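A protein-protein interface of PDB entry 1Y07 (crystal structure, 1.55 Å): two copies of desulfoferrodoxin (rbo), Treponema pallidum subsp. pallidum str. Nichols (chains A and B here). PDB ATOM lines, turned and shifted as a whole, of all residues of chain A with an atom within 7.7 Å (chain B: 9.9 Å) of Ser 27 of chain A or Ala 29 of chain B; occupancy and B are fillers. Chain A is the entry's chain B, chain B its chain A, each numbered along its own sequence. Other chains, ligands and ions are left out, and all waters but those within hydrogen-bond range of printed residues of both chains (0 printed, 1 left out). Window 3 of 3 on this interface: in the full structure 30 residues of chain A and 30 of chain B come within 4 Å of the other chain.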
ATOM      1  N   PHE A   8      22.135  21.878  18.829  1.00  0.00           N
ATOM      2  CA  PHE A   8      20.772  22.317  19.122  1.00  0.00           C
ATOM      3  C   PHE A   8      19.900  21.055  19.012  1.00  0.00           C
ATOM      4  O   PHE A   8      19.823  20.466  17.939  1.00  0.00           O
ATOM      5  CB  PHE A   8      20.323  23.357  18.099  1.00  0.00           C
ATOM      6  CG  PHE A   8      21.279  24.518  17.967  1.00  0.00           C
ATOM      7  CD1 PHE A   8      22.440  24.394  17.252  1.00  0.00           C
ATOM      8  CD2 PHE A   8      21.004  25.728  18.574  1.00  0.00           C
ATOM      9  CE1 PHE A   8      23.325  25.455  17.140  1.00  0.00           C
ATOM     10  CE2 PHE A   8      21.895  26.782  18.474  1.00  0.00           C
ATOM     11  CZ  PHE A   8      23.068  26.630  17.739  1.00  0.00           C
ATOM     12  N   ALA A  22      28.408  29.180  14.543  1.00  0.00           N
ATOM     13  CA  ALA A  22      27.200  29.886  14.947  1.00  0.00           C
ATOM     14  C   ALA A  22      27.616  31.089  15.815  1.00  0.00           C
ATOM     15  O   ALA A  22      28.307  30.954  16.828  1.00  0.00           O
ATOM     16  CB  ALA A  22      26.317  28.974  15.750  1.00  0.00           C
ATOM     17  N   PRO A  23      27.113  32.242  15.471  1.00  0.00           N
ATOM     18  CA  PRO A  23      27.210  33.412  16.348  1.00  0.00           C
ATOM     19  C   PRO A  23      26.549  33.174  17.706  1.00  0.00           C
ATOM     20  O   PRO A  23      25.527  32.481  17.710  1.00  0.00           O
ATOM     21  CB  PRO A  23      26.440  34.457  15.576  1.00  0.00           C
ATOM     22  CG  PRO A  23      26.497  34.005  14.197  1.00  0.00           C
ATOM     23  CD  PRO A  23      26.381  32.520  14.232  1.00  0.00           C
ATOM     24  N   ALA A  24      27.135  33.718  18.784  1.00  0.00           N
ATOM     25  CA  ALA A  24      26.662  33.653  20.167  1.00  0.00           C
ATOM     26  C   ALA A  24      25.196  33.967  20.227  1.00  0.00           C
ATOM     27  O   ALA A  24      24.737  34.898  19.560  1.00  0.00           O
ATOM     28  CB  ALA A  24      27.439  34.672  21.065  1.00  0.00           C
ATOM     29  N   GLY A  25      24.466  33.181  21.015  1.00  0.00           N
ATOM     30  CA  GLY A  25      23.015  33.397  21.128  1.00  0.00           C
ATOM     31  C   GLY A  25      22.149  32.934  19.931  1.00  0.00           C
ATOM     32  O   GLY A  25      20.926  33.157  19.899  1.00  0.00           O
ATOM     33  N   SER A  26      22.738  32.269  18.939  1.00  0.00           N
ATOM     34  CA  SER A  26      21.951  31.723  17.832  1.00  0.00           C
ATOM     35  C   SER A  26      20.909  30.758  18.396  1.00  0.00           C
ATOM     36  O   SER A  26      21.133  30.163  19.463  1.00  0.00           O
ATOM     37  CB  SER A  26      22.871  30.941  16.867  1.00  0.00           C
ATOM     38  OG  SER A  26      23.718  31.814  16.141  1.00  0.00           O
ATOM     39  N   SER A  27      19.831  30.575  17.645  1.00  0.00           N
ATOM     40  CA  SER A  27      18.788  29.629  17.982  1.00  0.00           C
ATOM     41  C   SER A  27      18.063  29.060  16.740  1.00  0.00           C
ATOM     42  O   SER A  27      18.233  29.539  15.611  1.00  0.00           O
ATOM     43  CB  SER A  27      17.789  30.330  18.917  1.00  0.00           C
ATOM     44  OG  SER A  27      17.172  31.383  18.235  1.00  0.00           O
ATOM     45  N   VAL A  28      17.336  27.976  16.966  1.00  0.00           N
ATOM     46  CA  VAL A  28      16.584  27.281  15.932  1.00  0.00           C
ATOM     47  C   VAL A  28      15.163  27.161  16.380  1.00  0.00           C
ATOM     48  O   VAL A  28      14.873  26.677  17.500  1.00  0.00           O
ATOM     49  CB  VAL A  28      17.099  25.850  15.713  1.00  0.00           C
ATOM     50  CG1 VAL A  28      16.446  25.237  14.498  1.00  0.00           C
ATOM     51  CG2 VAL A  28      18.605  25.854  15.588  1.00  0.00           C
ATOM     52  N   ALA A  29      14.258  27.619  15.527  1.00  0.00           N
ATOM     53  CA  ALA A  29      12.833  27.510  15.796  1.00  0.00           C
ATOM     54  C   ALA A  29      12.384  26.258  15.065  1.00  0.00           C
ATOM     55  O   ALA A  29      12.599  26.130  13.877  1.00  0.00           O
ATOM     56  CB  ALA A  29      12.127  28.706  15.259  1.00  0.00           C
ATOM     57  N   CYS A  30      11.801  25.313  15.767  1.00  0.00           N
ATOM     58  CA  CYS A  30      11.563  24.018  15.141  1.00  0.00           C
ATOM     59  C   CYS A  30      10.372  23.343  15.856  1.00  0.00           C
ATOM     60  O   CYS A  30      10.502  22.782  16.944  1.00  0.00           O
ATOM     61  CB  CYS A  30      12.940  23.266  15.082  1.00  0.00           C
ATOM     62  SG  CYS A  30      13.144  21.632  15.742  1.00  0.00           S
ATOM     63  N   VAL A  34      11.848  26.653  20.713  1.00  0.00           N
ATOM     64  CA  VAL A  34      13.028  27.426  20.284  1.00  0.00           C
ATOM     65  C   VAL A  34      14.212  26.710  20.915  1.00  0.00           C
ATOM     66  O   VAL A  34      14.279  26.545  22.142  1.00  0.00           O
ATOM     67  CB  VAL A  34      12.931  28.917  20.717  1.00  0.00           C
ATOM     68  CG1 VAL A  34      14.237  29.640  20.535  1.00  0.00           C
ATOM     69  CG2 VAL A  34      11.852  29.614  19.912  1.00  0.00           C
ATOM     70  N   LEU A  35      15.164  26.263  20.098  1.00  0.00           N
ATOM     71  CA  LEU A  35      16.281  25.478  20.594  1.00  0.00           C
ATOM     72  C   LEU A  35      17.458  26.448  20.717  1.00  0.00           C
ATOM     73  O   LEU A  35      17.657  27.244  19.827  1.00  0.00           O
ATOM     74  CB  LEU A  35      16.667  24.384  19.624  1.00  0.00           C
ATOM     75  CG  LEU A  35      15.549  23.461  19.130  1.00  0.00           C
ATOM     76  CD1 LEU A  35      16.174  22.452  18.154  1.00  0.00           C
ATOM     77  CD2 LEU A  35      14.812  22.785  20.241  1.00  0.00           C
ATOM     78  N   ARG A  36      18.151  26.399  21.844  1.00  0.00           N
ATOM     79  CA  ARG A  36      19.365  27.175  22.051  1.00  0.00           C
ATOM     80  C   ARG A  36      20.561  26.236  22.074  1.00  0.00           C
ATOM     81  O   ARG A  36      20.436  25.072  22.362  1.00  0.00           O
ATOM     82  CB  ARG A  36      19.328  27.937  23.389  1.00  0.00           C
ATOM     83  CG  ARG A  36      18.117  28.841  23.618  1.00  0.00           C
ATOM     84  CD  ARG A  36      18.136  30.108  22.805  1.00  0.00           C
ATOM     85  NE  ARG A  36      16.882  30.859  22.926  1.00  0.00           N
ATOM     86  CZ  ARG A  36      16.684  32.056  22.382  1.00  0.00           C
ATOM     87  NH1 ARG A  36      15.513  32.668  22.528  1.00  0.00           N
ATOM     88  NH2 ARG A  36      17.658  32.651  21.705  1.00  0.00           N
ATOM     89  N   ALA A  37      21.762  26.772  21.849  1.00  0.00           N
ATOM     90  CA  ALA A  37      22.957  25.932  21.902  1.00  0.00           C
ATOM     91  C   ALA A  37      23.058  25.327  23.289  1.00  0.00           C
ATOM     92  O   ALA A  37      23.020  26.048  24.326  1.00  0.00           O
ATOM     93  CB  ALA A  37      24.183  26.776  21.614  1.00  0.00           C
ATOM     94  N   PHE B   8      21.364  24.605   6.320  1.00  0.00           N
ATOM     95  CA  PHE B   8      20.998  26.009   6.579  1.00  0.00           C
ATOM     96  C   PHE B   8      22.288  26.848   6.433  1.00  0.00           C
ATOM     97  O   PHE B   8      23.254  26.647   7.158  1.00  0.00           O
ATOM     98  CB  PHE B   8      20.433  26.116   7.964  1.00  0.00           C
ATOM     99  CG  PHE B   8      19.261  25.185   8.192  1.00  0.00           C
ATOM    100  CD1 PHE B   8      19.447  23.835   8.508  1.00  0.00           C
ATOM    101  CD2 PHE B   8      17.943  25.698   8.120  1.00  0.00           C
ATOM    102  CE1 PHE B   8      18.329  22.982   8.690  1.00  0.00           C
ATOM    103  CE2 PHE B   8      16.826  24.857   8.318  1.00  0.00           C
ATOM    104  CZ  PHE B   8      17.017  23.508   8.611  1.00  0.00           C
ATOM    105  N   GLN B  10      24.495  30.218   6.196  1.00  0.00           N
ATOM    106  CA  GLN B  10      24.767  31.626   6.462  1.00  0.00           C
ATOM    107  C   GLN B  10      25.620  32.246   5.369  1.00  0.00           C
ATOM    108  O   GLN B  10      25.346  33.386   4.986  1.00  0.00           O
ATOM    109  CB  GLN B  10      25.443  31.774   7.833  1.00  0.00           C
ATOM    110  CG  GLN B  10      26.695  30.894   8.022  1.00  0.00           C
ATOM    111  CD  GLN B  10      26.527  29.757   9.008  1.00  0.00           C
ATOM    112  OE1 GLN B  10      27.062  29.799  10.130  1.00  0.00           O
ATOM    113  NE2 GLN B  10      25.833  28.718   8.592  1.00  0.00           N
ATOM    114  N   PHE B  17      24.804  25.436   9.237  1.00  0.00           N
ATOM    115  CA  PHE B  17      24.139  24.495  10.140  1.00  0.00           C
ATOM    116  C   PHE B  17      23.707  23.274   9.336  1.00  0.00           C
ATOM    117  O   PHE B  17      23.171  23.406   8.289  1.00  0.00           O
ATOM    118  CB  PHE B  17      22.918  25.061  10.850  1.00  0.00           C
ATOM    119  CG  PHE B  17      23.195  26.286  11.636  1.00  0.00           C
ATOM    120  CD1 PHE B  17      23.474  27.465  10.970  1.00  0.00           C
ATOM    121  CD2 PHE B  17      23.194  26.258  13.015  1.00  0.00           C
ATOM    122  CE1 PHE B  17      23.739  28.632  11.662  1.00  0.00           C
ATOM    123  CE2 PHE B  17      23.464  27.449  13.747  1.00  0.00           C
ATOM    124  CZ  PHE B  17      23.751  28.620  13.048  1.00  0.00           C
ATOM    125  N   GLY B  25      10.077  23.728   7.559  1.00  0.00           N
ATOM    126  CA  GLY B  25       9.733  25.001   8.143  1.00  0.00           C
ATOM    127  C   GLY B  25      10.559  25.394   9.347  1.00  0.00           C
ATOM    128  O   GLY B  25      10.334  26.451   9.888  1.00  0.00           O
ATOM    129  N   SER B  26      11.567  24.607   9.716  1.00  0.00           N
ATOM    130  CA  SER B  26      12.538  25.027  10.724  1.00  0.00           C
ATOM    131  C   SER B  26      13.246  26.279  10.218  1.00  0.00           C
ATOM    132  O   SER B  26      13.494  26.420   9.013  1.00  0.00           O
ATOM    133  CB  SER B  26      13.613  23.963  10.917  1.00  0.00           C
ATOM    134  OG  SER B  26      13.094  22.807  11.526  1.00  0.00           O
ATOM    135  N   SER B  27      13.624  27.137  11.143  1.00  0.00           N
ATOM    136  CA  SER B  27      14.505  28.232  10.805  1.00  0.00           C
ATOM    137  C   SER B  27      15.589  28.414  11.860  1.00  0.00           C
ATOM    138  O   SER B  27      15.414  28.089  13.032  1.00  0.00           O
ATOM    139  CB  SER B  27      13.683  29.498  10.608  1.00  0.00           C
ATOM    140  OG  SER B  27      13.155  30.018  11.810  1.00  0.00           O
ATOM    141  N   VAL B  28      16.700  28.963  11.440  1.00  0.00           N
ATOM    142  CA  VAL B  28      17.797  29.229  12.341  1.00  0.00           C
ATOM    143  C   VAL B  28      18.070  30.710  12.433  1.00  0.00           C
ATOM    144  O   VAL B  28      18.358  31.350  11.421  1.00  0.00           O
ATOM    145  CB  VAL B  28      19.093  28.562  11.847  1.00  0.00           C
ATOM    146  CG1 VAL B  28      20.245  28.936  12.760  1.00  0.00           C
ATOM    147  CG2 VAL B  28      18.877  27.021  11.730  1.00  0.00           C
ATOM    148  N   ALA B  29      17.978  31.266  13.634  1.00  0.00           N
ATOM    149  CA  ALA B  29      18.518  32.622  13.888  1.00  0.00           C
ATOM    150  C   ALA B  29      20.018  32.511  14.159  1.00  0.00           C
ATOM    151  O   ALA B  29      20.441  32.095  15.255  1.00  0.00           O
ATOM    152  CB  ALA B  29      17.851  33.232  15.040  1.00  0.00           C
ATOM    153  N   CYS B  30      20.805  32.872  13.142  1.00  0.00           N
ATOM    154  CA  CYS B  30      22.234  32.680  13.153  1.00  0.00           C
ATOM    155  C   CYS B  30      22.771  34.046  13.379  1.00  0.00           C
ATOM    156  O   CYS B  30      23.010  34.798  12.412  1.00  0.00           O
ATOM    157  CB  CYS B  30      22.699  32.118  11.809  1.00  0.00           C
ATOM    158  SG  CYS B  30      24.540  31.993  11.622  1.00  0.00           S
ATOM    159  N   GLY B  31      22.928  34.387  14.655  1.00  0.00           N
ATOM    160  CA  GLY B  31      23.172  35.762  15.029  1.00  0.00           C
ATOM    161  C   GLY B  31      21.938  36.529  14.619  1.00  0.00           C
ATOM    162  O   GLY B  31      20.827  36.192  15.065  1.00  0.00           O
ATOM    163  N   SER B  32      22.133  37.535  13.768  1.00  0.00           N
ATOM    164  CA  SER B  32      21.036  38.363  13.249  1.00  0.00           C
ATOM    165  C   SER B  32      20.538  37.930  11.866  1.00  0.00           C
ATOM    166  O   SER B  32      19.704  38.594  11.285  1.00  0.00           O
ATOM    167  CB  SER B  32      21.485  39.824  13.173  1.00  0.00           C
ATOM    168  OG  SER B  32      22.463  40.000  12.160  1.00  0.00           O
ATOM    169  N   GLU B  33      21.060  36.825  11.329  1.00  0.00           N
ATOM    170  CA  GLU B  33      20.595  36.257  10.069  1.00  0.00           C
ATOM    171  C   GLU B  33      19.461  35.255  10.403  1.00  0.00           C
ATOM    172  O   GLU B  33      19.424  34.708  11.526  1.00  0.00           O
ATOM    173  CB  GLU B  33      21.789  35.553   9.362  1.00  0.00           C
ATOM    174  CG  GLU B  33      22.283  36.202   8.080  1.00  0.00           C
ATOM    175  CD  GLU B  33      23.371  35.372   7.384  1.00  0.00           C
ATOM    176  OE1 GLU B  33      24.397  35.075   8.044  1.00  0.00           O
ATOM    177  OE2 GLU B  33      23.218  35.016   6.186  1.00  0.00           O
ATOM    178  N   VAL B  34      18.507  35.052   9.493  1.00  0.00           N
ATOM    179  CA  VAL B  34      17.639  33.857   9.587  1.00  0.00           C
ATOM    180  C   VAL B  34      17.887  32.907   8.409  1.00  0.00           C
ATOM    181  O   VAL B  34      17.937  33.360   7.261  1.00  0.00           O
ATOM    182  CB  VAL B  34      16.158  34.187   9.647  1.00  0.00           C
ATOM    183  CG1 VAL B  34      15.311  32.928   9.599  1.00  0.00           C
ATOM    184  CG2 VAL B  34      15.840  34.891  10.972  1.00  0.00           C
ATOM    185  N   LEU B  35      18.001  31.620   8.695  1.00  0.00           N
ATOM    186  CA  LEU B  35      18.347  30.618   7.665  1.00  0.00           C
ATOM    187  C   LEU B  35      17.219  29.591   7.588  1.00  0.00           C
ATOM    188  O   LEU B  35      16.732  29.142   8.606  1.00  0.00           O
ATOM    189  CB  LEU B  35      19.673  29.915   8.015  1.00  0.00           C
ATOM    190  CG  LEU B  35      20.873  30.787   8.411  1.00  0.00           C
ATOM    191  CD1 LEU B  35      22.015  29.933   8.961  1.00  0.00           C
ATOM    192  CD2 LEU B  35      21.269  31.608   7.236  1.00  0.00           C
ATOM    193  N   ARG B  36      16.765  29.261   6.377  1.00  0.00           N
ATOM    194  CA  ARG B  36      15.892  28.116   6.166  1.00  0.00           C
ATOM    195  C   ARG B  36      16.594  27.047   5.296  1.00  0.00           C
ATOM    196  O   ARG B  36      17.616  27.315   4.679  1.00  0.00           O
ATOM    197  CB  ARG B  36      14.634  28.526   5.492  1.00  0.00           C
ATOM    198  CG  ARG B  36      13.670  29.211   6.462  1.00  0.00           C
ATOM    199  CD  ARG B  36      12.286  29.456   5.902  1.00  0.00           C
ATOM    200  NE  ARG B  36      11.429  30.061   6.910  1.00  0.00           N
ATOM    201  CZ  ARG B  36      11.582  31.299   7.327  1.00  0.00           C
ATOM    202  NH1 ARG B  36      12.568  32.066   6.828  1.00  0.00           N
ATOM    203  NH2 ARG B  36      10.755  31.786   8.255  1.00  0.00           N
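Of chain B, only Val 28 and Ala 29 come within 4 Å of Ser 27 of chain A. Ala 29 of chain B touches two residues of chain A. Ser 26 of chain A touches just these residues of chain B: Ala 29 (3.0 Å), Cys 30 (3.4 Å) and Gly 31 (3.1 Å). Printed residues of chain B within 4 Å of Ala 29 of chain A: Ser 26 and Ser 27. Of the printed residues of chain A, Ser 26 of chain B touches Ala 29 (3.3 Å) and Cys 30 (3.6 Å). Of the printed residues of chain B, Cys 30 of chain A touches Ser 26. Printed residues of chain A within 4 Å of Gly 31 of chain B: Pro 23 (3.6 Å) and Ser 26 (3.1 Å). Printed residues of chain B within 4 Å of Phe 8 of chain A: Phe 17. The nearest residue of chain A that does not touch Ala 29 of chain B is Val 28 of chain A (4.7 Å).
Of the 14 printed residues of chain A, 8 touch a printed residue of chain B. Hydrophobic or aromatic side chains of chain A within 4 Å of the printed part of chain B: Phe 8, Ala 22, Pro 23, Val 28 and Ala 29. Of the 15 printed residues of chain B, 7 touch a printed residue of chain A. Printed residues of chain B that touch a printed residue of chain A: Phe 17, Ser 26, Ser 27, Val 28, Ala 29, Cys 30 and Gly 31. Hydrophobic or aromatic side chains of chain B that line the printed part of chain A: Phe 17, Val 28 and Ala 29. Among the printed residues, 13 pairs touch across the chains.
N of Ala 29 of chain A is in hydrogen-bond range of O of Ser 27 of chain B (2.8 Å). O of Ala 29 of chain B sits close to OG of Ser 26 of chain A, 3.4 Å away. The backbone carbonyl oxygen (O) of Ser 27 of chain A sits at hydrogen-bond distance from the backbone NH (N) of Ala 29 of chain B, at 2.6 Å. N of Gly 31 of chain B is in hydrogen-bond range of OG of Ser 26 of chain A, 3.1 Å away.
Ser 26 of chain A touches Ala 29 of chain B, and with the chains exchanged Ala 29 of chain A touches Ser 26 of chain B. Ser 26 of chain A touches Cys 30 of chain B, and with the chains exchanged Cys 30 of chain A touches Ser 26 of chain B. Ser 27 of chain A touches Val 28 of chain B, and with the chains exchanged Val 28 of chain A touches Ser 27 of chain B. Ser 27 of chain A touches Ala 29 of chain B, and with the chains exchanged Ala 29 of chain A touches Ser 27 of chain B. 10 positions are printed for both chains. Of the 13 pairs that touch across the chains among the printed residues, 8 have their exchanged pair printed and touching as well.
Among the printed residues, pairs that only touch across the chains: Phe 8 of chain A with Phe 17 of chain B (3.9 Å), Ala 22 of chain A with Phe 17 of chain B (3.7 Å), Pro 23 of chain A with Cys 30 of chain B (3.2 Å), Pro 23 of chain A with Gly 31 of chain B (3.6 Å), Ser 26 of chain A with Cys 30 of chain B (3.4 Å), Ser 27 of chain A with Val 28 of chain B (3.3 Å), Val 28 of chain A with Ser 27 of chain B (3.2 Å), Ala 29 of chain A with Ser 26 of chain B (3.3 Å) and Cys 30 of chain A with Ser 26 of chain B (3.6 Å).
The backbone NH (N) of Phe 17 of chain B is in hydrogen-bond range of the backbone carbonyl oxygen (O) of Phe 8 of chain B (2.9 Å). OE1 of Gln 10 of chain B lies within hydrogen-bond range of SG of Cys 30 of chain B, 3.7 Å away. The backbone carbonyl oxygen of Val 28 of chain B sits at hydrogen-bond distance from the backbone NH of Leu 35 of chain B. The side-chain hydroxyl of Ser 26 of chain A is in hydrogen-bond range of the backbone carbonyl oxygen of Pro 23 of chain A. O of Val 28 of chain A lies within hydrogen-bond range of N of Leu 35 of chain A.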
